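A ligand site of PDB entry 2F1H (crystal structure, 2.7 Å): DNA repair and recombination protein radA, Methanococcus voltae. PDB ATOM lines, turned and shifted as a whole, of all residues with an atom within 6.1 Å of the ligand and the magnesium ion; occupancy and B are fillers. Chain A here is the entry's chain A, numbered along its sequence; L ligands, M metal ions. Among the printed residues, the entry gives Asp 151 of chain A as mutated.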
ATOM      1  N   GLY A 105      34.424 -20.845  -3.551  1.00  0.00           N
ATOM      2  CA  GLY A 105      34.790 -19.607  -2.892  1.00  0.00           C
ATOM      3  C   GLY A 105      35.793 -19.735  -1.765  1.00  0.00           C
ATOM      4  O   GLY A 105      36.001 -20.801  -1.194  1.00  0.00           O
ATOM      5  N   VAL A 106      36.424 -18.606  -1.470  1.00  0.00           N
ATOM      6  CA  VAL A 106      37.444 -18.472  -0.437  1.00  0.00           C
ATOM      7  C   VAL A 106      36.983 -18.990   0.923  1.00  0.00           C
ATOM      8  O   VAL A 106      35.784 -19.166   1.150  1.00  0.00           O
ATOM      9  CB  VAL A 106      37.876 -16.980  -0.301  1.00  0.00           C
ATOM     10  CG1 VAL A 106      36.704 -16.139   0.140  1.00  0.00           C
ATOM     11  CG2 VAL A 106      39.025 -16.850   0.660  1.00  0.00           C
ATOM     12  N   PHE A 107      37.931 -19.213   1.821  1.00  0.00           N
ATOM     13  CA  PHE A 107      37.605 -19.707   3.138  1.00  0.00           C
ATOM     14  C   PHE A 107      36.632 -18.768   3.849  1.00  0.00           C
ATOM     15  O   PHE A 107      36.710 -17.546   3.712  1.00  0.00           O
ATOM     16  CB  PHE A 107      38.876 -19.885   3.975  1.00  0.00           C
ATOM     17  CG  PHE A 107      39.381 -18.609   4.587  1.00  0.00           C
ATOM     18  CD1 PHE A 107      38.858 -18.153   5.807  1.00  0.00           C
ATOM     19  CD2 PHE A 107      40.355 -17.852   3.946  1.00  0.00           C
ATOM     20  CE1 PHE A 107      39.295 -16.958   6.362  1.00  0.00           C
ATOM     21  CE2 PHE A 107      40.792 -16.652   4.492  1.00  0.00           C
ATOM     22  CZ  PHE A 107      40.258 -16.197   5.699  1.00  0.00           C
ATOM     23  N   GLY A 108      35.706 -19.345   4.608  1.00  0.00           N
ATOM     24  CA  GLY A 108      34.742 -18.576   5.355  1.00  0.00           C
ATOM     25  C   GLY A 108      33.740 -17.750   4.571  1.00  0.00           C
ATOM     26  O   GLY A 108      33.143 -16.846   5.141  1.00  0.00           O
ATOM     27  N   SER A 109      33.547 -18.051   3.286  1.00  0.00           N
ATOM     28  CA  SER A 109      32.588 -17.262   2.506  1.00  0.00           C
ATOM     29  C   SER A 109      31.130 -17.668   2.706  1.00  0.00           C
ATOM     30  O   SER A 109      30.228 -17.037   2.152  1.00  0.00           O
ATOM     31  CB  SER A 109      32.953 -17.284   1.022  1.00  0.00           C
ATOM     32  OG  SER A 109      33.176 -18.608   0.567  1.00  0.00           O
ATOM     33  N   GLY A 110      30.910 -18.712   3.510  1.00  0.00           N
ATOM     34  CA  GLY A 110      29.572 -19.206   3.844  1.00  0.00           C
ATOM     35  C   GLY A 110      29.058 -20.468   3.157  1.00  0.00           C
ATOM     36  O   GLY A 110      27.894 -20.819   3.289  1.00  0.00           O
ATOM     37  N   LYS A 111      29.927 -21.151   2.419  1.00  0.00           N
ATOM     38  CA  LYS A 111      29.576 -22.347   1.671  1.00  0.00           C
ATOM     39  C   LYS A 111      28.887 -23.399   2.509  1.00  0.00           C
ATOM     40  O   LYS A 111      27.895 -24.005   2.082  1.00  0.00           O
ATOM     41  CB  LYS A 111      30.819 -22.952   1.029  1.00  0.00           C
ATOM     42  CG  LYS A 111      31.590 -21.998   0.149  1.00  0.00           C
ATOM     43  CD  LYS A 111      32.754 -22.688  -0.542  1.00  0.00           C
ATOM     44  CE  LYS A 111      33.858 -23.063   0.429  1.00  0.00           C
ATOM     45  NZ  LYS A 111      34.377 -21.883   1.148  1.00  0.00           N
ATOM     46  N   THR A 112      29.423 -23.635   3.690  1.00  0.00           N
ATOM     47  CA  THR A 112      28.890 -24.625   4.606  1.00  0.00           C
ATOM     48  C   THR A 112      27.585 -24.181   5.200  1.00  0.00           C
ATOM     49  O   THR A 112      26.692 -24.994   5.434  1.00  0.00           O
ATOM     50  CB  THR A 112      29.889 -24.877   5.702  1.00  0.00           C
ATOM     51  OG1 THR A 112      31.068 -25.449   5.123  1.00  0.00           O
ATOM     52  CG2 THR A 112      29.297 -25.822   6.735  1.00  0.00           C
ATOM     53  N   GLN A 113      27.483 -22.888   5.457  1.00  0.00           N
ATOM     54  CA  GLN A 113      26.279 -22.281   6.009  1.00  0.00           C
ATOM     55  C   GLN A 113      25.112 -22.501   5.062  1.00  0.00           C
ATOM     56  O   GLN A 113      23.996 -22.750   5.487  1.00  0.00           O
ATOM     57  CB  GLN A 113      26.499 -20.785   6.187  1.00  0.00           C
ATOM     58  CG  GLN A 113      27.723 -20.455   6.984  1.00  0.00           C
ATOM     59  CD  GLN A 113      27.655 -21.051   8.356  1.00  0.00           C
ATOM     60  OE1 GLN A 113      26.769 -20.731   9.137  1.00  0.00           O
ATOM     61  NE2 GLN A 113      28.589 -21.960   8.656  1.00  0.00           N
ATOM     62  N   ILE A 114      25.374 -22.394   3.768  1.00  0.00           N
ATOM     63  CA  ILE A 114      24.346 -22.575   2.752  1.00  0.00           C
ATOM     64  C   ILE A 114      23.866 -24.012   2.716  1.00  0.00           C
ATOM     65  O   ILE A 114      22.697 -24.284   2.447  1.00  0.00           O
ATOM     66  CB  ILE A 114      24.881 -22.147   1.377  1.00  0.00           C
ATOM     67  CG1 ILE A 114      25.090 -20.630   1.378  1.00  0.00           C
ATOM     68  CG2 ILE A 114      23.922 -22.543   0.280  1.00  0.00           C
ATOM     69  CD1 ILE A 114      25.822 -20.105   0.201  1.00  0.00           C
ATOM     70  N   ASP A 151      34.825 -32.498   4.865  1.00  0.00           N
ATOM     71  CA  ASP A 151      35.772 -31.762   5.702  1.00  0.00           C
ATOM     72  C   ASP A 151      35.654 -32.100   7.196  1.00  0.00           C
ATOM     73  O   ASP A 151      36.570 -31.887   7.973  1.00  0.00           O
ATOM     74  CB  ASP A 151      35.579 -30.248   5.556  1.00  0.00           C
ATOM     75  CG  ASP A 151      35.330 -29.813   4.123  1.00  0.00           C
ATOM     76  OD1 ASP A 151      35.882 -30.418   3.180  1.00  0.00           O
ATOM     77  OD2 ASP A 151      34.588 -28.823   3.953  1.00  0.00           O
ATOM     78  N   THR A 153      32.998 -30.886   8.939  1.00  0.00           N
ATOM     79  CA  THR A 153      32.455 -29.648   9.499  1.00  0.00           C
ATOM     80  C   THR A 153      30.955 -29.596   9.770  1.00  0.00           C
ATOM     81  O   THR A 153      30.413 -28.528  10.069  1.00  0.00           O
ATOM     82  CB  THR A 153      32.804 -28.453   8.625  1.00  0.00           C
ATOM     83  OG1 THR A 153      32.699 -28.815   7.238  1.00  0.00           O
ATOM     84  CG2 THR A 153      34.210 -27.962   8.947  1.00  0.00           C
ATOM     85  N   ARG A 158      24.319 -25.722  14.774  1.00  0.00           N
ATOM     86  CA  ARG A 158      23.935 -24.818  13.707  1.00  0.00           C
ATOM     87  C   ARG A 158      22.584 -25.191  13.073  1.00  0.00           C
ATOM     88  O   ARG A 158      21.805 -24.319  12.706  1.00  0.00           O
ATOM     89  CB  ARG A 158      25.053 -24.796  12.677  1.00  0.00           C
ATOM     90  CG  ARG A 158      25.079 -23.587  11.792  1.00  0.00           C
ATOM     91  CD  ARG A 158      24.999 -22.297  12.571  1.00  0.00           C
ATOM     92  NE  ARG A 158      25.104 -21.151  11.665  1.00  0.00           N
ATOM     93  CZ  ARG A 158      24.586 -19.951  11.920  1.00  0.00           C
ATOM     94  NH1 ARG A 158      24.739 -18.981  11.027  1.00  0.00           N
ATOM     95  NH2 ARG A 158      23.925 -19.728  13.040  1.00  0.00           N
ATOM     96  N   GLN A 161      20.035 -24.233  15.720  1.00  0.00           N
ATOM     97  CA  GLN A 161      19.977 -22.789  15.768  1.00  0.00           C
ATOM     98  C   GLN A 161      19.165 -22.192  14.621  1.00  0.00           C
ATOM     99  O   GLN A 161      18.217 -21.432  14.855  1.00  0.00           O
ATOM    100  CB  GLN A 161      21.397 -22.236  15.764  1.00  0.00           C
ATOM    101  CG  GLN A 161      21.465 -20.743  15.641  1.00  0.00           C
ATOM    102  CD  GLN A 161      22.801 -20.206  16.045  1.00  0.00           C
ATOM    103  OE1 GLN A 161      23.845 -20.704  15.618  1.00  0.00           O
ATOM    104  NE2 GLN A 161      22.787 -19.168  16.874  1.00  0.00           N
ATOM    105  N   ASP A 211      29.964 -31.594   0.829  1.00  0.00           N
ATOM    106  CA  ASP A 211      30.787 -30.504   1.366  1.00  0.00           C
ATOM    107  C   ASP A 211      31.977 -31.095   2.102  1.00  0.00           C
ATOM    108  O   ASP A 211      31.784 -31.658   3.163  1.00  0.00           O
ATOM    109  CB  ASP A 211      29.924 -29.662   2.322  1.00  0.00           C
ATOM    110  CG  ASP A 211      30.674 -28.487   2.918  1.00  0.00           C
ATOM    111  OD1 ASP A 211      31.463 -27.834   2.217  1.00  0.00           O
ATOM    112  OD2 ASP A 211      30.433 -28.201   4.105  1.00  0.00           O
ATOM    113  N   THR A 255      29.926 -27.865  -2.638  1.00  0.00           N
ATOM    114  CA  THR A 255      30.811 -26.737  -2.367  1.00  0.00           C
ATOM    115  C   THR A 255      32.184 -27.036  -2.982  1.00  0.00           C
ATOM    116  O   THR A 255      32.559 -28.191  -3.187  1.00  0.00           O
ATOM    117  CB  THR A 255      30.948 -26.491  -0.849  1.00  0.00           C
ATOM    118  OG1 THR A 255      31.520 -27.633  -0.222  1.00  0.00           O
ATOM    119  CG2 THR A 255      29.608 -26.235  -0.235  1.00  0.00           C
ATOM    120  N   GLN A 257      36.464 -25.413  -3.502  1.00  0.00           N
ATOM    121  CA  GLN A 257      37.488 -24.476  -3.113  1.00  0.00           C
ATOM    122  C   GLN A 257      38.007 -23.731  -4.337  1.00  0.00           C
ATOM    123  O   GLN A 257      37.766 -24.143  -5.472  1.00  0.00           O
ATOM    124  CB  GLN A 257      38.615 -25.228  -2.425  1.00  0.00           C
ATOM    125  CG  GLN A 257      38.114 -26.364  -1.575  1.00  0.00           C
ATOM    126  CD  GLN A 257      39.192 -26.921  -0.650  1.00  0.00           C
ATOM    127  OE1 GLN A 257      40.366 -27.013  -1.035  1.00  0.00           O
ATOM    128  NE2 GLN A 257      38.791 -27.317   0.557  1.00  0.00           N
ATOM    129  N   VAL A 288      31.239 -17.228  -4.210  1.00  0.00           N
ATOM    130  CA  VAL A 288      30.793 -16.469  -3.053  1.00  0.00           C
ATOM    131  C   VAL A 288      31.933 -15.650  -2.443  1.00  0.00           C
ATOM    132  O   VAL A 288      33.043 -16.155  -2.264  1.00  0.00           O
ATOM    133  CB  VAL A 288      30.216 -17.394  -1.982  1.00  0.00           C
ATOM    134  CG1 VAL A 288      28.842 -17.869  -2.374  1.00  0.00           C
ATOM    135  CG2 VAL A 288      31.144 -18.586  -1.802  1.00  0.00           C
ATOM    136  N   ARG A 296      27.621 -10.836   2.341  1.00  0.00           N
ATOM    137  CA  ARG A 296      28.201 -11.774   1.380  1.00  0.00           C
ATOM    138  C   ARG A 296      27.674 -11.517  -0.024  1.00  0.00           C
ATOM    139  O   ARG A 296      26.642 -10.877  -0.194  1.00  0.00           O
ATOM    140  CB  ARG A 296      27.833 -13.217   1.766  1.00  0.00           C
ATOM    141  CG  ARG A 296      28.332 -13.665   3.119  1.00  0.00           C
ATOM    142  CD  ARG A 296      29.775 -14.098   3.043  1.00  0.00           C
ATOM    143  NE  ARG A 296      30.329 -14.257   4.381  1.00  0.00           N
ATOM    144  CZ  ARG A 296      30.694 -13.255   5.163  1.00  0.00           C
ATOM    145  NH1 ARG A 296      30.578 -11.997   4.734  1.00  0.00           N
ATOM    146  NH2 ARG A 296      31.158 -13.494   6.372  1.00  0.00           N
ATOM    147  N   ILE A 315      25.139 -13.436   6.705  1.00  0.00           N
ATOM    148  CA  ILE A 315      25.274 -14.643   7.500  1.00  0.00           C
ATOM    149  C   ILE A 315      25.202 -14.209   8.962  1.00  0.00           C
ATOM    150  O   ILE A 315      26.152 -13.624   9.490  1.00  0.00           O
ATOM    151  CB  ILE A 315      26.619 -15.352   7.265  1.00  0.00           C
ATOM    152  CG1 ILE A 315      26.806 -15.665   5.783  1.00  0.00           C
ATOM    153  CG2 ILE A 315      26.681 -16.632   8.101  1.00  0.00           C
ATOM    154  CD1 ILE A 315      25.901 -16.758   5.260  1.00  0.00           C
ATOM    155  N   THR A 316      24.079 -14.471   9.616  1.00  0.00           N
ATOM    156  CA  THR A 316      23.912 -14.093  11.010  1.00  0.00           C
ATOM    157  C   THR A 316      23.630 -15.308  11.855  1.00  0.00           C
ATOM    158  O   THR A 316      23.810 -16.437  11.412  1.00  0.00           O
ATOM    159  CB  THR A 316      22.763 -13.098  11.206  1.00  0.00           C
ATOM    160  OG1 THR A 316      21.526 -13.814  11.197  1.00  0.00           O
ATOM    161  CG2 THR A 316      22.756 -12.078  10.081  1.00  0.00           C
ATOM    162  N   GLU A 317      23.184 -15.092  13.086  1.00  0.00           N
ATOM    163  CA  GLU A 317      22.891 -16.208  13.969  1.00  0.00           C
ATOM    164  C   GLU A 317      21.673 -16.969  13.482  1.00  0.00           C
ATOM    165  O   GLU A 317      21.435 -18.109  13.881  1.00  0.00           O
ATOM    166  CB  GLU A 317      22.689 -15.704  15.403  1.00  0.00           C
ATOM    167  CG  GLU A 317      22.515 -14.182  15.537  1.00  0.00           C
ATOM    168  CD  GLU A 317      21.090 -13.713  15.270  1.00  0.00           C
ATOM    169  OE1 GLU A 317      20.160 -14.194  15.958  1.00  0.00           O
ATOM    170  OE2 GLU A 317      20.906 -12.851  14.373  1.00  0.00           O
ATOM    171  N   LYS A 318      20.906 -16.335  12.600  1.00  0.00           N
ATOM    172  CA  LYS A 318      19.705 -16.952  12.052  1.00  0.00           C
ATOM    173  C   LYS A 318      20.010 -17.740  10.780  1.00  0.00           C
ATOM    174  O   LYS A 318      19.151 -18.430  10.254  1.00  0.00           O
ATOM    175  CB  LYS A 318      18.671 -15.872  11.744  1.00  0.00           C
ATOM    176  CG  LYS A 318      18.371 -14.994  12.930  1.00  0.00           C
ATOM    177  CD  LYS A 318      17.368 -13.909  12.605  1.00  0.00           C
ATOM    178  CE  LYS A 318      17.145 -13.005  13.803  1.00  0.00           C
ATOM    179  NZ  LYS A 318      16.332 -11.825  13.436  1.00  0.00           N
HETATM  180  P1  LIG L   1      35.649 -23.141   4.102  1.00  0.00           P
HETATM  181  O1  LIG L   1      35.262 -24.010   3.046  1.00  0.00           O
HETATM  182  O2  LIG L   1      35.628 -23.901   5.376  1.00  0.00           O
HETATM  183  O3  LIG L   1      36.976 -22.669   3.861  1.00  0.00           O
HETATM  184  P2  LIG L   1      33.063 -21.908   4.467  1.00  0.00           P
HETATM  185  O4  LIG L   1      32.594 -23.313   4.583  1.00  0.00           O
HETATM  186  O5  LIG L   1      32.379 -21.238   3.390  1.00  0.00           O
HETATM  187  N1  LIG L   1      34.619 -21.830   4.201  1.00  0.00           N
HETATM  188  P3  LIG L   1      31.369 -21.209   6.641  1.00  0.00           P
HETATM  189  O6  LIG L   1      30.272 -21.705   5.705  1.00  0.00           O
HETATM  190  O7  LIG L   1      31.498 -22.126   7.771  1.00  0.00           O
HETATM  191  O8  LIG L   1      32.788 -21.137   5.849  1.00  0.00           O
HETATM  192  O9  LIG L   1      31.005 -19.673   7.204  1.00  0.00           O
HETATM  193  C1  LIG L   1      31.902 -19.012   8.249  1.00  0.00           C
HETATM  194  C2  LIG L   1      31.304 -17.958   8.830  1.00  0.00           C
HETATM  195  O10 LIG L   1      29.973 -18.333   9.334  1.00  0.00           O
HETATM  196  C3  LIG L   1      32.051 -17.592  10.173  1.00  0.00           C
HETATM  197  O11 LIG L   1      33.339 -17.121  10.022  1.00  0.00           O
HETATM  198  C4  LIG L   1      30.963 -16.901  11.025  1.00  0.00           C
HETATM  199  O12 LIG L   1      31.055 -15.376  10.807  1.00  0.00           O
HETATM  200  C5  LIG L   1      29.653 -17.436  10.424  1.00  0.00           C
HETATM  201  N2  LIG L   1      28.967 -18.063  11.387  1.00  0.00           N
HETATM  202  C6  LIG L   1      29.022 -19.418  11.726  1.00  0.00           C
HETATM  203  N3  LIG L   1      28.223 -19.632  12.724  1.00  0.00           N
HETATM  204  C7  LIG L   1      27.630 -18.468  13.079  1.00  0.00           C
HETATM  205  C8  LIG L   1      26.723 -18.123  14.051  1.00  0.00           C
HETATM  206  N4  LIG L   1      26.232 -19.046  14.906  1.00  0.00           N
HETATM  207  N5  LIG L   1      26.300 -16.783  14.154  1.00  0.00           N
HETATM  208  C9  LIG L   1      26.802 -15.795  13.270  1.00  0.00           C
HETATM  209  N6  LIG L   1      27.706 -16.103  12.297  1.00  0.00           N
HETATM  210  C10 LIG L   1      28.092 -17.483  12.249  1.00  0.00           C
HETATM  211 MG    MG M   1      33.350 -25.325   5.001  1.00  0.00          MG
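The backbone NH (N) of Thr 112 sits at hydrogen-bond distance from an oxygen (O6) of the ligand. The backbone NH of Gly 110 is in hydrogen-bond range of an oxygen (O5) of the ligand (2.9 Å). The backbone NH (N) of Gly 108 sits close to a nitrogen (N1) of the ligand, at 2.7 Å. OE1 of Gln 161 sits at hydrogen-bond distance from N4 of the ligand, 3.0 Å away. The backbone NH (N) of Gln 113 is in hydrogen-bond range of an oxygen (O6) of the ligand, at 3.0 Å. O5 of the ligand lies within hydrogen-bond range of N of Lys 111 (2.6 Å). N of Ser 109 sits at hydrogen-bond distance from O5 of the ligand (3.4 Å). An oxygen (O1) of the ligand is in salt-bridge range of the side-chain amino group (NZ) of Lys 111, 3.0 Å away. An oxygen (O7) of the ligand is in hydrogen-bond range of the side-chain amide nitrogen (NE2) of Gln 113 (3.0 Å).
OD2 of Asp 211 sits close to OG1 of Thr 112. The side-chain amino group (NZ) of Lys 111 sits at hydrogen-bond distance from the backbone carbonyl oxygen (O) of Val 106 (3.1 Å). The side-chain hydroxyl (OG1) of Thr 316 lies within hydrogen-bond range of the backbone NH (N) of Lys 318 (3.0 Å). The side-chain hydroxyl (OG) of Ser 109 lies within hydrogen-bond range of the backbone carbonyl oxygen (O) of Val 106, 2.7 Å away. The backbone carbonyl oxygen (O) of Glu 317 is in hydrogen-bond range of the guanidinium group (NH2) of Arg 158 (3.1 Å). The side-chain amide oxygen (OE1) of Gln 113 sits at hydrogen-bond distance from the guanidinium group (NE) of Arg 158, 3.1 Å away. NH2 of Arg 158 lies within hydrogen-bond range of OE1 of Gln 161. The guanidinium group (NH1) of Arg 158 lies within hydrogen-bond range of the backbone carbonyl oxygen (O) of Thr 316, 2.7 Å away.
N4 of the ligand sits close to NH2 of Arg 158 (3.0 Å). Phe 107 touches the ligand. CG2 of Ile 315 touches C5 of the ligand, at 3.9 Å. Thr 316 touches the ligand. Glu 317 touches the ligand. Hydrophobic or aromatic side chains within 4 Å of the ligand: Phe 107 and Ile 315. 12 residues have an atom within 4 Å of the ligand: Phe 107, Gly 108, Ser 109, Gly 110, Lys 111, Thr 112, Gln 113, Arg 158, Gln 161, Ile 315, Thr 316 and Glu 317.
Residues that only touch the magnesium ion: Asp 151 (3.9 Å). Two residues have an atom within 4 Å of the magnesium ion: Thr 112 and Asp 151. The nearest printed residue that does not touch the magnesium ion is Asp 211 (4.2 Å).
The magnesium ion is bound by O4 of the ligand (2.2 Å) and OG1 of Thr 112 (2.3 Å). Slightly farther from the magnesium ion lies an oxygen (O2) of the ligand (2.7 Å).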
